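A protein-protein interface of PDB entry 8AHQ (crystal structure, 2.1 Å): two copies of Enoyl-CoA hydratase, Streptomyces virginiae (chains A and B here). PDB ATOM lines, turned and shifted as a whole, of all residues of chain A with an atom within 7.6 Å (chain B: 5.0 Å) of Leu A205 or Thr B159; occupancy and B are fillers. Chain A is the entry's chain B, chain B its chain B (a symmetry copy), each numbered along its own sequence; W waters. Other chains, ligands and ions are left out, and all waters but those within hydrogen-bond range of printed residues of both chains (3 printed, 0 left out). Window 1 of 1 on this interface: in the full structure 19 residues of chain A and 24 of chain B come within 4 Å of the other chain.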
ATOM      1  N   THR A  92     -25.441 -16.588   8.569  1.00  0.00           N
ATOM      2  CA  THR A  92     -26.284 -15.399   8.286  1.00  0.00           C
ATOM      3  C   THR A  92     -27.359 -15.237   9.353  1.00  0.00           C
ATOM      4  O   THR A  92     -27.830 -14.107   9.475  1.00  0.00           O
ATOM      5  CB  THR A  92     -26.999 -15.431   6.917  1.00  0.00           C
ATOM      6  OG1 THR A  92     -28.078 -16.375   6.928  1.00  0.00           O
ATOM      7  CG2 THR A  92     -26.062 -15.707   5.760  1.00  0.00           C
ATOM      8  N   ARG A 196     -19.212  -2.494  21.699  1.00  0.00           N
ATOM      9  CA  ARG A 196     -20.152  -1.382  22.003  1.00  0.00           C
ATOM     10  C   ARG A 196     -21.594  -1.885  21.968  1.00  0.00           C
ATOM     11  O   ARG A 196     -22.448  -1.240  22.535  1.00  0.00           O
ATOM     12  CB  ARG A 196     -20.059  -0.275  20.936  1.00  0.00           C
ATOM     13  CG  ARG A 196     -18.725   0.461  20.926  1.00  0.00           C
ATOM     14  CD  ARG A 196     -18.505   1.339  19.707  1.00  0.00           C
ATOM     15  NE  ARG A 196     -18.737   0.654  18.443  1.00  0.00           N
ATOM     16  CZ  ARG A 196     -18.692   1.273  17.276  1.00  0.00           C
ATOM     17  NH1 ARG A 196     -18.359   2.551  17.251  1.00  0.00           N
ATOM     18  NH2 ARG A 196     -18.946   0.621  16.154  1.00  0.00           N
ATOM     19  N   THR A 197     -21.907  -2.923  21.193  1.00  0.00           N
ATOM     20  CA  THR A 197     -23.293  -3.420  21.137  1.00  0.00           C
ATOM     21  C   THR A 197     -23.324  -4.749  21.889  1.00  0.00           C
ATOM     22  O   THR A 197     -22.410  -4.994  22.690  1.00  0.00           O
ATOM     23  CB  THR A 197     -23.821  -3.401  19.706  1.00  0.00           C
ATOM     24  OG1 THR A 197     -25.214  -3.695  19.817  1.00  0.00           O
ATOM     25  CG2 THR A 197     -23.129  -4.394  18.800  1.00  0.00           C
ATOM     26  N   ARG A 199     -25.340  -9.036  22.057  1.00  0.00           N
ATOM     27  CA  ARG A 199     -25.835 -10.205  21.296  1.00  0.00           C
ATOM     28  C   ARG A 199     -27.322 -10.064  20.926  1.00  0.00           C
ATOM     29  O   ARG A 199     -27.725 -10.449  19.785  1.00  0.00           O
ATOM     30  CB  ARG A 199     -25.598 -11.440  22.157  1.00  0.00           C
ATOM     31  CG  ARG A 199     -26.156 -12.712  21.568  1.00  0.00           C
ATOM     32  CD  ARG A 199     -25.426 -13.915  22.135  1.00  0.00           C
ATOM     33  NE  ARG A 199     -26.183 -15.140  21.911  1.00  0.00           N
ATOM     34  CZ  ARG A 199     -25.740 -16.374  22.144  1.00  0.00           C
ATOM     35  NH1 ARG A 199     -24.498 -16.578  22.558  1.00  0.00           N
ATOM     36  NH2 ARG A 199     -26.545 -17.399  21.940  1.00  0.00           N
ATOM     37  N   SER A 200     -28.133  -9.600  21.873  1.00  0.00           N
ATOM     38  CA  SER A 200     -29.580  -9.385  21.660  1.00  0.00           C
ATOM     39  C   SER A 200     -29.813  -8.428  20.450  1.00  0.00           C
ATOM     40  O   SER A 200     -30.696  -8.696  19.617  1.00  0.00           O
ATOM     41  CB  SER A 200     -30.198  -8.878  22.923  1.00  0.00           C
ATOM     42  OG  SER A 200     -31.486  -8.373  22.668  1.00  0.00           O
ATOM     43  N   THR A 201     -29.014  -7.375  20.350  1.00  0.00           N
ATOM     44  CA  THR A 201     -29.128  -6.309  19.314  1.00  0.00           C
ATOM     45  C   THR A 201     -28.622  -6.903  17.981  1.00  0.00           C
ATOM     46  O   THR A 201     -29.300  -6.743  16.942  1.00  0.00           O
ATOM     47  CB  THR A 201     -28.401  -5.033  19.767  1.00  0.00           C
ATOM     48  OG1 THR A 201     -28.943  -4.535  21.003  1.00  0.00           O
ATOM     49  CG2 THR A 201     -28.474  -3.948  18.716  1.00  0.00           C
ATOM     50  N   THR A 202     -27.496  -7.618  18.006  1.00  0.00           N
ATOM     51  CA  THR A 202     -26.941  -8.286  16.796  1.00  0.00           C
ATOM     52  C   THR A 202     -27.957  -9.318  16.295  1.00  0.00           C
ATOM     53  O   THR A 202     -28.176  -9.371  15.070  1.00  0.00           O
ATOM     54  CB  THR A 202     -25.538  -8.819  17.088  1.00  0.00           C
ATOM     55  OG1 THR A 202     -24.745  -7.727  17.548  1.00  0.00           O
ATOM     56  CG2 THR A 202     -24.866  -9.403  15.873  1.00  0.00           C
ATOM     57  N   ALA A 203     -28.549 -10.099  17.200  1.00  0.00           N
ATOM     58  CA  ALA A 203     -29.559 -11.139  16.907  1.00  0.00           C
ATOM     59  C   ALA A 203     -30.748 -10.478  16.212  1.00  0.00           C
ATOM     60  O   ALA A 203     -31.181 -10.923  15.117  1.00  0.00           O
ATOM     61  CB  ALA A 203     -30.003 -11.866  18.169  1.00  0.00           C
ATOM     62  N   ALA A 204     -31.240  -9.380  16.762  1.00  0.00           N
ATOM     63  CA  ALA A 204     -32.450  -8.773  16.162  1.00  0.00           C
ATOM     64  C   ALA A 204     -32.118  -8.195  14.757  1.00  0.00           C
ATOM     65  O   ALA A 204     -32.918  -8.384  13.834  1.00  0.00           O
ATOM     66  CB  ALA A 204     -32.997  -7.807  17.165  1.00  0.00           C
ATOM     67  N   LEU A 205     -30.927  -7.622  14.574  1.00  0.00           N
ATOM     68  CA  LEU A 205     -30.456  -6.994  13.302  1.00  0.00           C
ATOM     69  C   LEU A 205     -30.420  -8.050  12.177  1.00  0.00           C
ATOM     70  O   LEU A 205     -31.032  -7.851  11.109  1.00  0.00           O
ATOM     71  CB  LEU A 205     -29.066  -6.379  13.531  1.00  0.00           C
ATOM     72  CG  LEU A 205     -28.516  -5.680  12.282  1.00  0.00           C
ATOM     73  CD1 LEU A 205     -29.435  -4.547  11.862  1.00  0.00           C
ATOM     74  CD2 LEU A 205     -27.128  -5.166  12.501  1.00  0.00           C
ATOM     75  N   LYS A 206     -29.807  -9.184  12.477  1.00  0.00           N
ATOM     76  CA  LYS A 206     -29.671 -10.319  11.541  1.00  0.00           C
ATOM     77  C   LYS A 206     -31.032 -10.924  11.267  1.00  0.00           C
ATOM     78  O   LYS A 206     -31.247 -11.287  10.115  1.00  0.00           O
ATOM     79  CB  LYS A 206     -28.647 -11.310  12.075  1.00  0.00           C
ATOM     80  CG  LYS A 206     -27.261 -10.703  12.236  1.00  0.00           C
ATOM     81  CD  LYS A 206     -26.265 -11.713  12.757  1.00  0.00           C
ATOM     82  CE  LYS A 206     -26.158 -12.896  11.807  1.00  0.00           C
ATOM     83  NZ  LYS A 206     -24.969 -13.724  12.106  1.00  0.00           N
ATOM     84  N   GLU A 207     -31.890 -11.052  12.290  1.00  0.00           N
ATOM     85  CA  GLU A 207     -33.277 -11.539  12.076  1.00  0.00           C
ATOM     86  C   GLU A 207     -33.992 -10.555  11.130  1.00  0.00           C
ATOM     87  O   GLU A 207     -34.732 -10.967  10.254  1.00  0.00           O
ATOM     88  CB  GLU A 207     -34.010 -11.644  13.414  1.00  0.00           C
ATOM     89  CG  GLU A 207     -35.345 -12.344  13.317  1.00  0.00           C
ATOM     90  CD  GLU A 207     -35.210 -13.866  13.257  1.00  0.00           C
ATOM     91  OE1 GLU A 207     -34.106 -14.389  12.860  1.00  0.00           O
ATOM     92  OE2 GLU A 207     -36.191 -14.541  13.649  1.00  0.00           O
ATOM     93  N   TYR A 208     -33.783  -9.264  11.284  1.00  0.00           N
ATOM     94  CA  TYR A 208     -34.478  -8.274  10.433  1.00  0.00           C
ATOM     95  C   TYR A 208     -33.865  -8.320   9.025  1.00  0.00           C
ATOM     96  O   TYR A 208     -34.595  -8.143   8.048  1.00  0.00           O
ATOM     97  CB  TYR A 208     -34.439  -6.888  11.072  1.00  0.00           C
ATOM     98  CG  TYR A 208     -35.191  -5.853  10.287  1.00  0.00           C
ATOM     99  CD1 TYR A 208     -36.551  -5.992  10.119  1.00  0.00           C
ATOM    100  CD2 TYR A 208     -34.566  -4.740   9.743  1.00  0.00           C
ATOM    101  CE1 TYR A 208     -37.291  -5.052   9.441  1.00  0.00           C
ATOM    102  CE2 TYR A 208     -35.295  -3.785   9.040  1.00  0.00           C
ATOM    103  CZ  TYR A 208     -36.660  -3.954   8.883  1.00  0.00           C
ATOM    104  OH  TYR A 208     -37.482  -3.079   8.248  1.00  0.00           O
ATOM    105  N   ARG A 209     -32.572  -8.573   8.885  1.00  0.00           N
ATOM    106  CA  ARG A 209     -32.039  -8.731   7.502  1.00  0.00           C
ATOM    107  C   ARG A 209     -32.788  -9.854   6.766  1.00  0.00           C
ATOM    108  O   ARG A 209     -33.100  -9.672   5.596  1.00  0.00           O
ATOM    109  CB  ARG A 209     -30.539  -9.007   7.497  1.00  0.00           C
ATOM    110  CG  ARG A 209     -29.949  -9.100   6.109  1.00  0.00           C
ATOM    111  CD  ARG A 209     -28.450  -9.105   6.208  1.00  0.00           C
ATOM    112  NE  ARG A 209     -27.896  -9.066   4.868  1.00  0.00           N
ATOM    113  CZ  ARG A 209     -26.618  -8.854   4.595  1.00  0.00           C
ATOM    114  NH1 ARG A 209     -25.745  -8.700   5.575  1.00  0.00           N
ATOM    115  NH2 ARG A 209     -26.216  -8.836   3.341  1.00  0.00           N
ATOM    116  N   ALA A 210     -33.034 -10.993   7.428  1.00  0.00           N
ATOM    117  CA  ALA A 210     -33.789 -12.134   6.855  1.00  0.00           C
ATOM    118  C   ALA A 210     -35.251 -11.720   6.575  1.00  0.00           C
ATOM    119  O   ALA A 210     -35.807 -12.189   5.568  1.00  0.00           O
ATOM    120  CB  ALA A 210     -33.714 -13.334   7.772  1.00  0.00           C
ATOM    121  N   ARG A 211     -35.824 -10.831   7.378  1.00  0.00           N
ATOM    122  CA  ARG A 211     -37.191 -10.301   7.183  1.00  0.00           C
ATOM    123  C   ARG A 211     -37.220  -9.375   5.960  1.00  0.00           C
ATOM    124  O   ARG A 211     -38.244  -9.372   5.256  1.00  0.00           O
ATOM    125  CB  ARG A 211     -37.677  -9.560   8.434  1.00  0.00           C
ATOM    126  CG  ARG A 211     -38.948  -8.733   8.234  1.00  0.00           C
ATOM    127  CD  ARG A 211     -40.154  -9.636   8.059  1.00  0.00           C
ATOM    128  NE  ARG A 211     -41.439  -8.924   7.948  1.00  0.00           N
ATOM    129  CZ  ARG A 211     -41.941  -8.430   6.819  1.00  0.00           C
ATOM    130  NH1 ARG A 211     -41.276  -8.562   5.677  1.00  0.00           N
ATOM    131  NH2 ARG A 211     -43.119  -7.837   6.831  1.00  0.00           N
ATOM    132  N   LEU A 212     -36.124  -8.643   5.708  1.00  0.00           N
ATOM    133  CA  LEU A 212     -36.083  -7.631   4.611  1.00  0.00           C
ATOM    134  C   LEU A 212     -35.491  -8.222   3.327  1.00  0.00           C
ATOM    135  O   LEU A 212     -35.987  -7.861   2.241  1.00  0.00           O
ATOM    136  CB  LEU A 212     -35.236  -6.450   5.087  1.00  0.00           C
ATOM    137  CG  LEU A 212     -35.722  -5.074   4.640  1.00  0.00           C
ATOM    138  CD1 LEU A 212     -37.165  -4.851   5.067  1.00  0.00           C
ATOM    139  CD2 LEU A 212     -34.824  -3.978   5.191  1.00  0.00           C
ATOM    140  N   LEU B 130     -25.889   5.665  11.200  1.00  0.00           N
ATOM    141  CA  LEU B 130     -26.896   4.952  12.009  1.00  0.00           C
ATOM    142  C   LEU B 130     -26.219   4.554  13.317  1.00  0.00           C
ATOM    143  O   LEU B 130     -25.372   3.647  13.287  1.00  0.00           O
ATOM    144  CB  LEU B 130     -27.402   3.765  11.196  1.00  0.00           C
ATOM    145  CG  LEU B 130     -28.107   4.121   9.890  1.00  0.00           C
ATOM    146  CD1 LEU B 130     -28.264   2.882   9.048  1.00  0.00           C
ATOM    147  CD2 LEU B 130     -29.469   4.726  10.144  1.00  0.00           C
ATOM    148  N   VAL B 133     -27.386   0.654  16.900  1.00  0.00           N
ATOM    149  CA  VAL B 133     -26.929  -0.583  17.638  1.00  0.00           C
ATOM    150  C   VAL B 133     -26.138  -0.185  18.899  1.00  0.00           C
ATOM    151  O   VAL B 133     -26.065  -0.972  19.810  1.00  0.00           O
ATOM    152  CB  VAL B 133     -26.084  -1.581  16.808  1.00  0.00           C
ATOM    153  CG1 VAL B 133     -26.816  -1.980  15.541  1.00  0.00           C
ATOM    154  CG2 VAL B 133     -24.704  -1.057  16.517  1.00  0.00           C
ATOM    155  N   VAL B 138     -32.387  -1.715  16.632  1.00  0.00           N
ATOM    156  CA  VAL B 138     -32.378  -1.880  15.153  1.00  0.00           C
ATOM    157  C   VAL B 138     -33.093  -0.712  14.477  1.00  0.00           C
ATOM    158  O   VAL B 138     -34.245  -0.444  14.768  1.00  0.00           O
ATOM    159  CB  VAL B 138     -33.003  -3.230  14.751  1.00  0.00           C
ATOM    160  CG1 VAL B 138     -32.946  -3.413  13.229  1.00  0.00           C
ATOM    161  CG2 VAL B 138     -32.307  -4.393  15.442  1.00  0.00           C
ATOM    162  N   PRO B 139     -32.465   0.017  13.522  1.00  0.00           N
ATOM    163  CA  PRO B 139     -33.165   1.068  12.774  1.00  0.00           C
ATOM    164  C   PRO B 139     -34.043   0.436  11.683  1.00  0.00           C
ATOM    165  O   PRO B 139     -33.810   0.607  10.511  1.00  0.00           O
ATOM    166  CB  PRO B 139     -32.045   1.909  12.155  1.00  0.00           C
ATOM    167  CG  PRO B 139     -30.868   0.894  12.012  1.00  0.00           C
ATOM    168  CD  PRO B 139     -31.064  -0.136  13.108  1.00  0.00           C
ATOM    169  N   LEU B 143     -33.826   1.407   7.674  1.00  0.00           N
ATOM    170  CA  LEU B 143     -33.039   0.480   6.805  1.00  0.00           C
ATOM    171  C   LEU B 143     -33.648   0.259   5.398  1.00  0.00           C
ATOM    172  O   LEU B 143     -32.848   0.346   4.466  1.00  0.00           O
ATOM    173  CB  LEU B 143     -32.824  -0.850   7.538  1.00  0.00           C
ATOM    174  CG  LEU B 143     -31.366  -1.260   7.738  1.00  0.00           C
ATOM    175  CD1 LEU B 143     -30.430  -0.101   7.435  1.00  0.00           C
ATOM    176  CD2 LEU B 143     -31.138  -1.775   9.149  1.00  0.00           C
ATOM    177  N   ARG B 154     -24.107  -3.329   2.365  1.00  0.00           N
ATOM    178  CA  ARG B 154     -23.524  -2.090   2.948  1.00  0.00           C
ATOM    179  C   ARG B 154     -24.496  -1.481   3.992  1.00  0.00           C
ATOM    180  O   ARG B 154     -24.039  -0.927   4.985  1.00  0.00           O
ATOM    181  CB  ARG B 154     -23.033  -1.171   1.827  1.00  0.00           C
ATOM    182  CG  ARG B 154     -22.178  -0.036   2.368  1.00  0.00           C
ATOM    183  CD  ARG B 154     -21.056  -0.536   3.295  1.00  0.00           C
ATOM    184  NE  ARG B 154     -20.110   0.527   3.557  1.00  0.00           N
ATOM    185  CZ  ARG B 154     -19.219   0.936   2.666  1.00  0.00           C
ATOM    186  NH1 ARG B 154     -19.189   0.359   1.487  1.00  0.00           N
ATOM    187  NH2 ARG B 154     -18.379   1.929   2.942  1.00  0.00           N
ATOM    188  N   ALA B 155     -25.805  -1.605   3.845  1.00  0.00           N
ATOM    189  CA  ALA B 155     -26.772  -0.998   4.795  1.00  0.00           C
ATOM    190  C   ALA B 155     -26.708  -1.741   6.155  1.00  0.00           C
ATOM    191  O   ALA B 155     -26.644  -1.051   7.210  1.00  0.00           O
ATOM    192  CB  ALA B 155     -28.164  -0.986   4.213  1.00  0.00           C
ATOM    193  N   PHE B 156     -26.670  -3.086   6.140  1.00  0.00           N
ATOM    194  CA  PHE B 156     -26.600  -3.943   7.361  1.00  0.00           C
ATOM    195  C   PHE B 156     -25.207  -3.894   8.001  1.00  0.00           C
ATOM    196  O   PHE B 156     -25.167  -3.870   9.230  1.00  0.00           O
ATOM    197  CB  PHE B 156     -27.114  -5.353   7.065  1.00  0.00           C
ATOM    198  CG  PHE B 156     -28.617  -5.376   6.991  1.00  0.00           C
ATOM    199  CD1 PHE B 156     -29.292  -4.929   5.871  1.00  0.00           C
ATOM    200  CD2 PHE B 156     -29.355  -5.615   8.145  1.00  0.00           C
ATOM    201  CE1 PHE B 156     -30.676  -4.900   5.848  1.00  0.00           C
ATOM    202  CE2 PHE B 156     -30.740  -5.557   8.133  1.00  0.00           C
ATOM    203  CZ  PHE B 156     -31.402  -5.230   6.981  1.00  0.00           C
ATOM    204  N   ALA B 157     -24.108  -3.811   7.241  1.00  0.00           N
ATOM    205  CA  ALA B 157     -22.747  -3.724   7.822  1.00  0.00           C
ATOM    206  C   ALA B 157     -22.493  -2.306   8.378  1.00  0.00           C
ATOM    207  O   ALA B 157     -21.880  -2.155   9.448  1.00  0.00           O
ATOM    208  CB  ALA B 157     -21.716  -4.145   6.800  1.00  0.00           C
ATOM    209  N   ALA B 158     -23.011  -1.289   7.727  1.00  0.00           N
ATOM    210  CA  ALA B 158     -22.967   0.090   8.251  1.00  0.00           C
ATOM    211  C   ALA B 158     -23.776   0.204   9.542  1.00  0.00           C
ATOM    212  O   ALA B 158     -23.388   0.990  10.387  1.00  0.00           O
ATOM    213  CB  ALA B 158     -23.413   1.084   7.234  1.00  0.00           C
ATOM    214  N   THR B 159     -24.873  -0.527   9.683  1.00  0.00           N
ATOM    215  CA  THR B 159     -25.663  -0.553  10.930  1.00  0.00           C
ATOM    216  C   THR B 159     -24.869  -1.249  12.049  1.00  0.00           C
ATOM    217  O   THR B 159     -24.741  -0.675  13.152  1.00  0.00           O
ATOM    218  CB  THR B 159     -27.031  -1.196  10.675  1.00  0.00           C
ATOM    219  OG1 THR B 159     -27.745  -0.412   9.700  1.00  0.00           O
ATOM    220  CG2 THR B 159     -27.836  -1.360  11.954  1.00  0.00           C
ATOM    221  N   LEU B 160     -24.316  -2.436  11.778  1.00  0.00           N
ATOM    222  CA  LEU B 160     -23.599  -3.264  12.772  1.00  0.00           C
ATOM    223  C   LEU B 160     -22.373  -2.499  13.277  1.00  0.00           C
ATOM    224  O   LEU B 160     -22.059  -2.580  14.525  1.00  0.00           O
ATOM    225  CB  LEU B 160     -23.196  -4.605  12.150  1.00  0.00           C
ATOM    226  CG  LEU B 160     -22.513  -5.601  13.078  1.00  0.00           C
ATOM    227  CD1 LEU B 160     -23.404  -5.929  14.260  1.00  0.00           C
ATOM    228  CD2 LEU B 160     -22.128  -6.872  12.295  1.00  0.00           C
ATOM    229  N   ARG B 161     -21.765  -1.710  12.398  1.00  0.00           N
ATOM    230  CA  ARG B 161     -20.481  -1.046  12.696  1.00  0.00           C
ATOM    231  C   ARG B 161     -20.693   0.438  13.053  1.00  0.00           C
ATOM    232  O   ARG B 161     -19.683   1.097  13.348  1.00  0.00           O
ATOM    233  CB  ARG B 161     -19.527  -1.222  11.507  1.00  0.00           C
ATOM    234  CG  ARG B 161     -19.025  -2.654  11.300  1.00  0.00           C
ATOM    235  CD  ARG B 161     -18.207  -2.669  10.006  1.00  0.00           C
ATOM    236  NE  ARG B 161     -16.936  -1.996  10.281  1.00  0.00           N
ATOM    237  CZ  ARG B 161     -16.420  -1.003   9.554  1.00  0.00           C
ATOM    238  NH1 ARG B 161     -17.014  -0.594   8.444  1.00  0.00           N
ATOM    239  NH2 ARG B 161     -15.255  -0.497   9.884  1.00  0.00           N
ATOM    240  N   ALA B 162     -21.944   0.917  13.002  1.00  0.00           N
ATOM    241  CA  ALA B 162     -22.379   2.337  13.102  1.00  0.00           C
ATOM    242  C   ALA B 162     -21.426   3.202  12.268  1.00  0.00           C
ATOM    243  O   ALA B 162     -20.779   4.107  12.843  1.00  0.00           O
ATOM    244  CB  ALA B 162     -22.387   2.783  14.536  1.00  0.00           C
HETATM  245  O   HOH W   1     -16.972   0.970  13.514  1.00  0.00           O
HETATM  246  O   HOH W   2     -18.571   3.555  14.568  1.00  0.00           O
HETATM  247  O   HOH W   3     -19.518  -2.068  15.888  1.00  0.00           O
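Of the 17 printed residues of chain A, 7 touch a printed residue of chain B.
Printed residues of chain A that touch a printed residue of chain B: Arg A196, Thr A197, Thr A201, Thr A202, Ala A204, Leu A205 and Arg A209.
Hydrophobic or aromatic side chains of chain A within 4 Å of the printed part of chain B: Ala A204 and Leu A205.
Among the printed residues, 10 pairs touch across the chains.
Of the printed residues of chain B, Thr A202 touches Leu B160.
Printed residues of chain B within 4 Å of Leu A205: Val B138 (3.6 Å), Phe B156 (3.8 Å), Thr B159 (3.6 Å) and Leu B160 (3.99 Å).
Leu B130 touches none of the printed residues of chain A.
Printed residues of chain A within 4 Å of Val B138: Ala A204 (3.9 Å) and Leu A205 (3.6 Å).
No residue of chain A comes within 4 Å of Ala B158.
Of chain A, only Leu A205 comes within 4 Å of Thr B159.
Of the printed residues of chain A, Leu B160 touches Thr A202 (3.98 Å) and Leu A205 (3.99 Å).
The nearest printed residue of chain B that does not touch Leu A205 is Leu B143 (4.2 Å).
The nearest printed residue of chain A that does not touch Val B138 is Tyr A208 (4.1 Å).
Thr A201 touches Val B133.
Leu B160 touches Thr A202.
CG2 of Val B138 touches C of Ala A204, 3.9 Å away.
Val B138 touches Leu A205.
O of Leu A205 touches CE2 of Phe B156 (3.8 Å).
Leu A205 touches Thr B159.
Leu B160 touches Leu A205.
Phe B156 touches Arg A209 (CE2 to CA, 3.5 Å).
Water W1 lies within hydrogen-bond range of the backbone carbonyl oxygen (O) of Arg B161 (2.7 Å) and the guanidinium group (NH2) of Arg A196 (3.3 Å).
Water W3 bridges NH2 of Arg A196 (2.8 Å) and O of Leu B160 (2.9 Å).
Water W2 lies within hydrogen-bond range of the backbone carbonyl oxygen of Ala B162 (2.9 Å), the guanidinium group of Arg A196 (2.9 Å) and the backbone carbonyl oxygen of Arg B161 (3.0 Å).
No position is printed for both chains.
Of the 10 pairs that touch across the chains among the printed residues, none has its exchanged pair printed and touching as well.
The guanidinium group (NH2) of Arg A196 is in hydrogen-bond range of the backbone carbonyl oxygen (O) of Arg B161 (2.9 Å).
OG1 of Thr A197 is in hydrogen-bond range of O of Val B133 (2.9 Å).
The backbone carbonyl oxygen (O) of Ala B155 lies within hydrogen-bond range of the side-chain hydroxyl (OG1) of Thr B159 (2.8 Å).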
